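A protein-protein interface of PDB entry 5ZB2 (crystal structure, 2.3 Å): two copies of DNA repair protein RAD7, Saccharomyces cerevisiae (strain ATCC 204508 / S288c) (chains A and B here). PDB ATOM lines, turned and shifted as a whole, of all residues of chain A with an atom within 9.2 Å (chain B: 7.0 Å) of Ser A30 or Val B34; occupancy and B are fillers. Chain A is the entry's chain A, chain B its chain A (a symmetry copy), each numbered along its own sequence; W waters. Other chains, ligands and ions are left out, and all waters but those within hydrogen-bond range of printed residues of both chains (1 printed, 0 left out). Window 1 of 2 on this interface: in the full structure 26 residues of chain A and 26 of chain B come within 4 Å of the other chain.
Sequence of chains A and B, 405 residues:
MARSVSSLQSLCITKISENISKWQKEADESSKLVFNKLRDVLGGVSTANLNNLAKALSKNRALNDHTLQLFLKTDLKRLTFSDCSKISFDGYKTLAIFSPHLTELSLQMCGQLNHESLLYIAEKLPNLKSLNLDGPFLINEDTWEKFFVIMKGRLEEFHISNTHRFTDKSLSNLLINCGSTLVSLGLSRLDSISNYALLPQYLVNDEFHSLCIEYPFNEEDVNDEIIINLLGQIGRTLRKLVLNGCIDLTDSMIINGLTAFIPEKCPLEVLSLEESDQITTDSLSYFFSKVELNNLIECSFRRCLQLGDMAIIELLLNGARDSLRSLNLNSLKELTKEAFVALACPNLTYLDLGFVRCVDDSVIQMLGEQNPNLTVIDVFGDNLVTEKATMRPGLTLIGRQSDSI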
ATOM      1  N   ILE A  20      16.048 -39.182  -4.026  1.00  0.00           N
ATOM      2  CA  ILE A  20      15.348 -38.254  -3.141  1.00  0.00           C
ATOM      3  C   ILE A  20      16.168 -36.984  -2.973  1.00  0.00           C
ATOM      4  O   ILE A  20      15.641 -35.870  -3.072  1.00  0.00           O
ATOM      5  CB  ILE A  20      15.041 -38.916  -1.784  1.00  0.00           C
ATOM      6  CG1 ILE A  20      14.104 -40.113  -1.970  1.00  0.00           C
ATOM      7  CG2 ILE A  20      14.396 -37.909  -0.830  1.00  0.00           C
ATOM      8  CD1 ILE A  20      13.919 -40.951  -0.724  1.00  0.00           C
ATOM      9  N   TRP A  23      15.883 -34.913  -5.970  1.00  0.00           N
ATOM     10  CA  TRP A  23      14.524 -34.388  -6.010  1.00  0.00           C
ATOM     11  C   TRP A  23      14.313 -33.279  -4.983  1.00  0.00           C
ATOM     12  O   TRP A  23      13.465 -32.404  -5.192  1.00  0.00           O
ATOM     13  CB  TRP A  23      13.532 -35.529  -5.791  1.00  0.00           C
ATOM     14  CG  TRP A  23      12.164 -35.097  -5.380  1.00  0.00           C
ATOM     15  CD1 TRP A  23      11.100 -34.848  -6.197  1.00  0.00           C
ATOM     16  CD2 TRP A  23      11.705 -34.879  -4.044  1.00  0.00           C
ATOM     17  NE1 TRP A  23      10.007 -34.484  -5.451  1.00  0.00           N
ATOM     18  CE2 TRP A  23      10.353 -34.492  -4.125  1.00  0.00           C
ATOM     19  CE3 TRP A  23      12.306 -34.971  -2.785  1.00  0.00           C
ATOM     20  CZ2 TRP A  23       9.592 -34.202  -2.995  1.00  0.00           C
ATOM     21  CZ3 TRP A  23      11.552 -34.678  -1.668  1.00  0.00           C
ATOM     22  CH2 TRP A  23      10.209 -34.298  -1.779  1.00  0.00           C
ATOM     23  N   GLN A  24      15.062 -33.295  -3.874  1.00  0.00           N
ATOM     24  CA  GLN A  24      14.946 -32.226  -2.885  1.00  0.00           C
ATOM     25  C   GLN A  24      15.116 -30.861  -3.541  1.00  0.00           C
ATOM     26  O   GLN A  24      14.312 -29.948  -3.325  1.00  0.00           O
ATOM     27  CB  GLN A  24      15.988 -32.397  -1.777  1.00  0.00           C
ATOM     28  CG  GLN A  24      15.819 -33.612  -0.892  1.00  0.00           C
ATOM     29  CD  GLN A  24      14.771 -33.419   0.175  1.00  0.00           C
ATOM     30  OE1 GLN A  24      13.804 -32.683  -0.013  1.00  0.00           O
ATOM     31  NE2 GLN A  24      14.958 -34.080   1.308  1.00  0.00           N
ATOM     32  N   LYS A  25      16.171 -30.706  -4.344  1.00  0.00           N
ATOM     33  CA  LYS A  25      16.431 -29.419  -4.981  1.00  0.00           C
ATOM     34  C   LYS A  25      15.292 -29.022  -5.912  1.00  0.00           C
ATOM     35  O   LYS A  25      14.880 -27.858  -5.937  1.00  0.00           O
ATOM     36  CB  LYS A  25      17.760 -29.468  -5.732  1.00  0.00           C
ATOM     37  CG  LYS A  25      18.957 -29.696  -4.820  1.00  0.00           C
ATOM     38  CD  LYS A  25      20.274 -29.527  -5.561  1.00  0.00           C
ATOM     39  CE  LYS A  25      21.459 -29.693  -4.622  1.00  0.00           C
ATOM     40  NZ  LYS A  25      22.760 -29.482  -5.316  1.00  0.00           N
ATOM     41  N   GLU A  26      14.763 -29.976  -6.680  1.00  0.00           N
ATOM     42  CA  GLU A  26      13.572 -29.696  -7.477  1.00  0.00           C
ATOM     43  C   GLU A  26      12.427 -29.222  -6.590  1.00  0.00           C
ATOM     44  O   GLU A  26      11.773 -28.213  -6.883  1.00  0.00           O
ATOM     45  CB  GLU A  26      13.158 -30.941  -8.267  1.00  0.00           C
ATOM     46  CG  GLU A  26      11.965 -30.719  -9.196  1.00  0.00           C
ATOM     47  CD  GLU A  26      11.434 -32.009  -9.793  1.00  0.00           C
ATOM     48  OE1 GLU A  26      10.251 -32.036 -10.195  1.00  0.00           O
ATOM     49  OE2 GLU A  26      12.199 -32.993  -9.859  1.00  0.00           O
ATOM     50  N   ALA A  27      12.160 -29.947  -5.501  1.00  0.00           N
ATOM     51  CA  ALA A  27      11.105 -29.534  -4.583  1.00  0.00           C
ATOM     52  C   ALA A  27      11.409 -28.169  -3.981  1.00  0.00           C
ATOM     53  O   ALA A  27      10.499 -27.360  -3.759  1.00  0.00           O
ATOM     54  CB  ALA A  27      10.925 -30.579  -3.482  1.00  0.00           C
ATOM     55  N   ASP A  28      12.687 -27.890  -3.715  1.00  0.00           N
ATOM     56  CA  ASP A  28      13.056 -26.585  -3.183  1.00  0.00           C
ATOM     57  C   ASP A  28      12.677 -25.473  -4.154  1.00  0.00           C
ATOM     58  O   ASP A  28      12.226 -24.400  -3.736  1.00  0.00           O
ATOM     59  CB  ASP A  28      14.553 -26.549  -2.879  1.00  0.00           C
ATOM     60  CG  ASP A  28      14.963 -25.308  -2.112  1.00  0.00           C
ATOM     61  OD1 ASP A  28      14.905 -25.329  -0.864  1.00  0.00           O
ATOM     62  OD2 ASP A  28      15.342 -24.309  -2.756  1.00  0.00           O
ATOM     63  N   GLU A  29      12.837 -25.715  -5.457  1.00  0.00           N
ATOM     64  CA  GLU A  29      12.442 -24.717  -6.446  1.00  0.00           C
ATOM     65  C   GLU A  29      10.928 -24.578  -6.505  1.00  0.00           C
ATOM     66  O   GLU A  29      10.400 -23.462  -6.540  1.00  0.00           O
ATOM     67  CB  GLU A  29      13.000 -25.083  -7.822  1.00  0.00           C
ATOM     68  CG  GLU A  29      14.513 -25.242  -7.858  1.00  0.00           C
ATOM     69  CD  GLU A  29      15.239 -24.074  -7.219  1.00  0.00           C
ATOM     70  OE1 GLU A  29      14.721 -22.940  -7.289  1.00  0.00           O
ATOM     71  OE2 GLU A  29      16.324 -24.294  -6.640  1.00  0.00           O
ATOM     72  N   SER A  30      10.209 -25.702  -6.522  1.00  0.00           N
ATOM     73  CA  SER A  30       8.754 -25.624  -6.471  1.00  0.00           C
ATOM     74  C   SER A  30       8.287 -24.851  -5.246  1.00  0.00           C
ATOM     75  O   SER A  30       7.253 -24.177  -5.296  1.00  0.00           O
ATOM     76  CB  SER A  30       8.144 -27.023  -6.474  1.00  0.00           C
ATOM     77  OG  SER A  30       6.743 -26.949  -6.266  1.00  0.00           O
ATOM     78  N   SER A  31       9.031 -24.935  -4.142  1.00  0.00           N
ATOM     79  CA  SER A  31       8.702 -24.134  -2.968  1.00  0.00           C
ATOM     80  C   SER A  31       8.876 -22.648  -3.259  1.00  0.00           C
ATOM     81  O   SER A  31       8.058 -21.824  -2.835  1.00  0.00           O
ATOM     82  CB  SER A  31       9.575 -24.554  -1.787  1.00  0.00           C
ATOM     83  OG  SER A  31       9.446 -25.940  -1.525  1.00  0.00           O
ATOM     84  N   LYS A  32       9.938 -22.290  -3.985  1.00  0.00           N
ATOM     85  CA  LYS A  32      10.169 -20.895  -4.342  1.00  0.00           C
ATOM     86  C   LYS A  32       8.961 -20.308  -5.060  1.00  0.00           C
ATOM     87  O   LYS A  32       8.492 -19.215  -4.725  1.00  0.00           O
ATOM     88  CB  LYS A  32      11.425 -20.792  -5.212  1.00  0.00           C
ATOM     89  CG  LYS A  32      11.819 -19.379  -5.609  1.00  0.00           C
ATOM     90  CD  LYS A  32      13.083 -19.389  -6.458  1.00  0.00           C
ATOM     91  CE  LYS A  32      13.468 -17.994  -6.919  1.00  0.00           C
ATOM     92  NZ  LYS A  32      14.713 -18.001  -7.740  1.00  0.00           N
ATOM     93  N   LEU A  33       8.434 -21.034  -6.049  1.00  0.00           N
ATOM     94  CA  LEU A  33       7.288 -20.537  -6.803  1.00  0.00           C
ATOM     95  C   LEU A  33       6.065 -20.363  -5.909  1.00  0.00           C
ATOM     96  O   LEU A  33       5.318 -19.389  -6.052  1.00  0.00           O
ATOM     97  CB  LEU A  33       6.972 -21.489  -7.957  1.00  0.00           C
ATOM     98  CG  LEU A  33       8.122 -21.761  -8.927  1.00  0.00           C
ATOM     99  CD1 LEU A  33       7.736 -22.858  -9.908  1.00  0.00           C
ATOM    100  CD2 LEU A  33       8.518 -20.490  -9.665  1.00  0.00           C
ATOM    101  N   VAL A  34       5.843 -21.296  -4.980  1.00  0.00           N
ATOM    102  CA  VAL A  34       4.652 -21.229  -4.138  1.00  0.00           C
ATOM    103  C   VAL A  34       4.722 -20.028  -3.203  1.00  0.00           C
ATOM    104  O   VAL A  34       3.699 -19.407  -2.893  1.00  0.00           O
ATOM    105  CB  VAL A  34       4.473 -22.544  -3.356  1.00  0.00           C
ATOM    106  CG1 VAL A  34       3.237 -22.481  -2.470  1.00  0.00           C
ATOM    107  CG2 VAL A  34       4.350 -23.711  -4.311  1.00  0.00           C
ATOM    108  N   PHE A  35       5.923 -19.686  -2.729  1.00  0.00           N
ATOM    109  CA  PHE A  35       6.059 -18.524  -1.856  1.00  0.00           C
ATOM    110  C   PHE A  35       5.950 -17.228  -2.649  1.00  0.00           C
ATOM    111  O   PHE A  35       5.387 -16.242  -2.161  1.00  0.00           O
ATOM    112  CB  PHE A  35       7.380 -18.588  -1.085  1.00  0.00           C
ATOM    113  CG  PHE A  35       7.393 -19.623   0.007  1.00  0.00           C
ATOM    114  CD1 PHE A  35       6.576 -19.485   1.120  1.00  0.00           C
ATOM    115  CD2 PHE A  35       8.222 -20.731  -0.074  1.00  0.00           C
ATOM    116  CE1 PHE A  35       6.580 -20.436   2.130  1.00  0.00           C
ATOM    117  CE2 PHE A  35       8.233 -21.685   0.934  1.00  0.00           C
ATOM    118  CZ  PHE A  35       7.411 -21.536   2.037  1.00  0.00           C
ATOM    119  N   ASN A  36       6.473 -17.213  -3.880  1.00  0.00           N
ATOM    120  CA  ASN A  36       6.257 -16.063  -4.753  1.00  0.00           C
ATOM    121  C   ASN A  36       4.771 -15.853  -5.019  1.00  0.00           C
ATOM    122  O   ASN A  36       4.296 -14.714  -5.074  1.00  0.00           O
ATOM    123  CB  ASN A  36       7.007 -16.248  -6.073  1.00  0.00           C
ATOM    124  CG  ASN A  36       8.509 -16.109  -5.921  1.00  0.00           C
ATOM    125  OD1 ASN A  36       8.999 -15.502  -4.969  1.00  0.00           O
ATOM    126  ND2 ASN A  36       9.249 -16.663  -6.873  1.00  0.00           N
ATOM    127  N   LYS A  37       4.023 -16.944  -5.184  1.00  0.00           N
ATOM    128  CA  LYS A  37       2.585 -16.832  -5.413  1.00  0.00           C
ATOM    129  C   LYS A  37       1.909 -16.074  -4.277  1.00  0.00           C
ATOM    130  O   LYS A  37       1.107 -15.165  -4.513  1.00  0.00           O
ATOM    131  CB  LYS A  37       1.970 -18.223  -5.577  1.00  0.00           C
ATOM    132  CG  LYS A  37       0.469 -18.229  -5.859  1.00  0.00           C
ATOM    133  CD  LYS A  37       0.132 -17.561  -7.184  1.00  0.00           C
ATOM    134  CE  LYS A  37      -1.359 -17.645  -7.486  1.00  0.00           C
ATOM    135  NZ  LYS A  37      -1.708 -16.988  -8.779  1.00  0.00           N
ATOM    136  N   LYS A  73      12.000 -18.216   0.972  1.00  0.00           N
ATOM    137  CA  LYS A  73      12.435 -18.460  -0.402  1.00  0.00           C
ATOM    138  C   LYS A  73      12.563 -17.152  -1.189  1.00  0.00           C
ATOM    139  O   LYS A  73      11.967 -16.970  -2.252  1.00  0.00           O
ATOM    140  CB  LYS A  73      11.484 -19.435  -1.104  1.00  0.00           C
ATOM    141  CG  LYS A  73      11.553 -20.875  -0.589  1.00  0.00           C
ATOM    142  CD  LYS A  73      12.974 -21.447  -0.608  1.00  0.00           C
ATOM    143  CE  LYS A  73      13.631 -21.341  -1.978  1.00  0.00           C
ATOM    144  NZ  LYS A  73      15.045 -21.820  -1.953  1.00  0.00           N
ATOM    145  N   PHE A  98      14.890 -22.134   4.450  1.00  0.00           N
ATOM    146  CA  PHE A  98      14.353 -21.511   3.247  1.00  0.00           C
ATOM    147  C   PHE A  98      14.932 -20.123   2.969  1.00  0.00           C
ATOM    148  O   PHE A  98      14.364 -19.377   2.165  1.00  0.00           O
ATOM    149  CB  PHE A  98      12.828 -21.425   3.347  1.00  0.00           C
ATOM    150  CG  PHE A  98      12.124 -22.740   3.145  1.00  0.00           C
ATOM    151  CD1 PHE A  98      12.467 -23.579   2.098  1.00  0.00           C
ATOM    152  CD2 PHE A  98      11.102 -23.131   3.998  1.00  0.00           C
ATOM    153  CE1 PHE A  98      11.813 -24.780   1.908  1.00  0.00           C
ATOM    154  CE2 PHE A  98      10.448 -24.333   3.813  1.00  0.00           C
ATOM    155  CZ  PHE A  98      10.803 -25.157   2.767  1.00  0.00           C
ATOM    156  N   GLU B  29      -1.834 -28.261  -1.953  1.00  0.00           N
ATOM    157  CA  GLU B  29      -2.017 -29.006  -3.194  1.00  0.00           C
ATOM    158  C   GLU B  29      -0.726 -29.048  -3.998  1.00  0.00           C
ATOM    159  O   GLU B  29      -0.340 -30.101  -4.516  1.00  0.00           O
ATOM    160  CB  GLU B  29      -3.145 -28.391  -4.023  1.00  0.00           C
ATOM    161  CG  GLU B  29      -4.478 -28.310  -3.296  1.00  0.00           C
ATOM    162  CD  GLU B  29      -4.872 -29.624  -2.649  1.00  0.00           C
ATOM    163  OE1 GLU B  29      -4.514 -30.688  -3.195  1.00  0.00           O
ATOM    164  OE2 GLU B  29      -5.534 -29.590  -1.590  1.00  0.00           O
ATOM    165  N   SER B  30      -0.043 -27.908  -4.122  1.00  0.00           N
ATOM    166  CA  SER B  30       1.252 -27.915  -4.792  1.00  0.00           C
ATOM    167  C   SER B  30       2.207 -28.902  -4.133  1.00  0.00           C
ATOM    168  O   SER B  30       3.051 -29.494  -4.812  1.00  0.00           O
ATOM    169  CB  SER B  30       1.861 -26.516  -4.793  1.00  0.00           C
ATOM    170  OG  SER B  30       3.185 -26.556  -5.301  1.00  0.00           O
ATOM    171  N   SER B  31       2.087 -29.092  -2.818  1.00  0.00           N
ATOM    172  CA  SER B  31       2.894 -30.104  -2.143  1.00  0.00           C
ATOM    173  C   SER B  31       2.522 -31.502  -2.620  1.00  0.00           C
ATOM    174  O   SER B  31       3.397 -32.351  -2.823  1.00  0.00           O
ATOM    175  CB  SER B  31       2.718 -29.989  -0.630  1.00  0.00           C
ATOM    176  OG  SER B  31       3.032 -28.683  -0.178  1.00  0.00           O
ATOM    177  N   LYS B  32       1.224 -31.756  -2.805  1.00  0.00           N
ATOM    178  CA  LYS B  32       0.775 -33.056  -3.292  1.00  0.00           C
ATOM    179  C   LYS B  32       1.458 -33.412  -4.606  1.00  0.00           C
ATOM    180  O   LYS B  32       1.970 -34.525  -4.775  1.00  0.00           O
ATOM    181  CB  LYS B  32      -0.747 -33.042  -3.453  1.00  0.00           C
ATOM    182  CG  LYS B  32      -1.359 -34.360  -3.901  1.00  0.00           C
ATOM    183  CD  LYS B  32      -2.873 -34.240  -4.016  1.00  0.00           C
ATOM    184  CE  LYS B  32      -3.507 -35.526  -4.518  1.00  0.00           C
ATOM    185  NZ  LYS B  32      -4.990 -35.415  -4.620  1.00  0.00           N
ATOM    186  N   LEU B  33       1.485 -32.468  -5.549  1.00  0.00           N
ATOM    187  CA  LEU B  33       2.101 -32.732  -6.845  1.00  0.00           C
ATOM    188  C   LEU B  33       3.591 -33.023  -6.705  1.00  0.00           C
ATOM    189  O   LEU B  33       4.125 -33.904  -7.390  1.00  0.00           O
ATOM    190  CB  LEU B  33       1.878 -31.544  -7.780  1.00  0.00           C
ATOM    191  CG  LEU B  33       0.420 -31.137  -7.999  1.00  0.00           C
ATOM    192  CD1 LEU B  33       0.349 -29.839  -8.789  1.00  0.00           C
ATOM    193  CD2 LEU B  33      -0.349 -32.244  -8.705  1.00  0.00           C
ATOM    194  N   VAL B  34       4.281 -32.296  -5.823  1.00  0.00           N
ATOM    195  CA  VAL B  34       5.726 -32.473  -5.690  1.00  0.00           C
ATOM    196  C   VAL B  34       6.046 -33.846  -5.112  1.00  0.00           C
ATOM    197  O   VAL B  34       7.058 -34.462  -5.468  1.00  0.00           O
ATOM    198  CB  VAL B  34       6.328 -31.344  -4.833  1.00  0.00           C
ATOM    199  CG1 VAL B  34       7.832 -31.525  -4.684  1.00  0.00           C
ATOM    200  CG2 VAL B  34       6.041 -29.997  -5.461  1.00  0.00           C
ATOM    201  N   PHE B  35       5.202 -34.344  -4.204  1.00  0.00           N
ATOM    202  CA  PHE B  35       5.439 -35.669  -3.639  1.00  0.00           C
ATOM    203  C   PHE B  35       5.084 -36.762  -4.640  1.00  0.00           C
ATOM    204  O   PHE B  35       5.757 -37.797  -4.700  1.00  0.00           O
ATOM    205  CB  PHE B  35       4.654 -35.841  -2.336  1.00  0.00           C
ATOM    206  CG  PHE B  35       5.221 -35.060  -1.181  1.00  0.00           C
ATOM    207  CD1 PHE B  35       6.463 -35.384  -0.653  1.00  0.00           C
ATOM    208  CD2 PHE B  35       4.516 -34.007  -0.621  1.00  0.00           C
ATOM    209  CE1 PHE B  35       6.994 -34.668   0.409  1.00  0.00           C
ATOM    210  CE2 PHE B  35       5.041 -33.288   0.444  1.00  0.00           C
ATOM    211  CZ  PHE B  35       6.282 -33.620   0.959  1.00  0.00           C
ATOM    212  N   ASN B  36       4.035 -36.547  -5.442  1.00  0.00           N
ATOM    213  CA  ASN B  36       3.743 -37.475  -6.531  1.00  0.00           C
ATOM    214  C   ASN B  36       4.907 -37.543  -7.513  1.00  0.00           C
ATOM    215  O   ASN B  36       5.235 -38.618  -8.027  1.00  0.00           O
ATOM    216  CB  ASN B  36       2.465 -37.057  -7.258  1.00  0.00           C
ATOM    217  CG  ASN B  36       1.214 -37.307  -6.438  1.00  0.00           C
ATOM    218  OD1 ASN B  36       1.208 -38.126  -5.519  1.00  0.00           O
ATOM    219  ND2 ASN B  36       0.140 -36.605  -6.779  1.00  0.00           N
ATOM    220  N   LYS B  37       5.543 -36.403  -7.783  1.00  0.00           N
ATOM    221  CA  LYS B  37       6.687 -36.386  -8.690  1.00  0.00           C
ATOM    222  C   LYS B  37       7.782 -37.327  -8.205  1.00  0.00           C
ATOM    223  O   LYS B  37       8.323 -38.121  -8.981  1.00  0.00           O
ATOM    224  CB  LYS B  37       7.222 -34.960  -8.832  1.00  0.00           C
ATOM    225  CG  LYS B  37       8.403 -34.813  -9.791  1.00  0.00           C
ATOM    226  CD  LYS B  37       8.027 -35.169 -11.222  1.00  0.00           C
ATOM    227  CE  LYS B  37       9.194 -34.942 -12.175  1.00  0.00           C
ATOM    228  NZ  LYS B  37       8.844 -35.294 -13.582  1.00  0.00           N
ATOM    229  N   LEU B  38       8.119 -37.258  -6.914  1.00  0.00           N
ATOM    230  CA  LEU B  38       9.136 -38.153  -6.368  1.00  0.00           C
ATOM    231  C   LEU B  38       8.757 -39.613  -6.586  1.00  0.00           C
ATOM    232  O   LEU B  38       9.574 -40.419  -7.046  1.00  0.00           O
ATOM    233  CB  LEU B  38       9.340 -37.868  -4.878  1.00  0.00           C
ATOM    234  CG  LEU B  38      10.284 -38.812  -4.129  1.00  0.00           C
ATOM    235  CD1 LEU B  38      11.661 -38.805  -4.755  1.00  0.00           C
ATOM    236  CD2 LEU B  38      10.364 -38.430  -2.658  1.00  0.00           C
ATOM    237  N   ARG B  39       7.515 -39.974  -6.256  1.00  0.00           N
ATOM    238  CA  ARG B  39       7.079 -41.356  -6.432  1.00  0.00           C
ATOM    239  C   ARG B  39       7.059 -41.747  -7.905  1.00  0.00           C
ATOM    240  O   ARG B  39       7.467 -42.858  -8.265  1.00  0.00           O
ATOM    241  CB  ARG B  39       5.699 -41.555  -5.807  1.00  0.00           C
ATOM    242  CG  ARG B  39       5.705 -41.546  -4.285  1.00  0.00           C
ATOM    243  CD  ARG B  39       4.308 -41.774  -3.723  1.00  0.00           C
ATOM    244  NE  ARG B  39       3.462 -40.587  -3.838  1.00  0.00           N
ATOM    245  CZ  ARG B  39       3.313 -39.664  -2.891  1.00  0.00           C
ATOM    246  NH1 ARG B  39       3.951 -39.768  -1.731  1.00  0.00           N
ATOM    247  NH2 ARG B  39       2.517 -38.626  -3.103  1.00  0.00           N
HETATM  248  O   HOH W   1       4.451 -26.528  -7.765  1.00  0.00           O
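Ser A30 touches just these residues of chain B: Ser B30 (3.7 Å) and Val B34 (3.2 Å).
Of chain A, only Trp A23 (2.9 Å), Ala A27 (3.5 Å) and Ser A30 (3.2 Å) come within 4 Å of Val B34.
Printed residues of chain B within 4 Å of Val A34: Ser B30 (3.2 Å).
Of the printed residues of chain B, Glu A26 touches Lys B37 (3.4 Å).
Printed residues of chain A within 4 Å of Lys B37: Glu A26 (3.4 Å).
Printed residues of chain B within 4 Å of Trp A23: Val B34, Phe B35 and Leu B38.
Lys B32 touches none of the printed residues of chain A.
The nearest printed residue of chain A that does not touch Phe B35 is Ala A27 (6.9 Å).
The backbone carbonyl oxygen (O) of Ala A27 lies within hydrogen-bond range of the side-chain hydroxyl (OG) of Ser A31 (2.8 Å).
Water W1 bridges OG of Ser A30 (2.8 Å) and OG of Ser B30 (2.8 Å).
The backbone carbonyl oxygen of Val B34 lies within hydrogen-bond range of the indole nitrogen of Trp A23 (2.9 Å).
Hydrophobic or aromatic side chains of chain B within 4 Å of the printed part of chain A: Val B34, Phe B35 and Leu B38.
Along chain B the printed residues that touch a printed residue of chain A span positions 30 to 38.
Among the printed residues, 9 pairs touch across the chains.
Among the printed residues, merely in contact across the chains: Ser A30 with Val B34 (3.2 Å), Val A34 with Ser B30 (3.2 Å), Glu A26 with Lys B37 (3.4 Å), Ala A27 with Val B34 (3.5 Å), Trp A23 with Leu B38 (3.5 Å), Ser A30 with Ser B30 (3.7 Å), Trp A23 with Phe B35 (3.9 Å) and Ile A20 with Leu B38 (3.9 Å).
Ser A30 touches its own counterpart, Ser B30.
Ser A30 touches Val B34, and with the chains exchanged Val A34 touches Ser B30.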
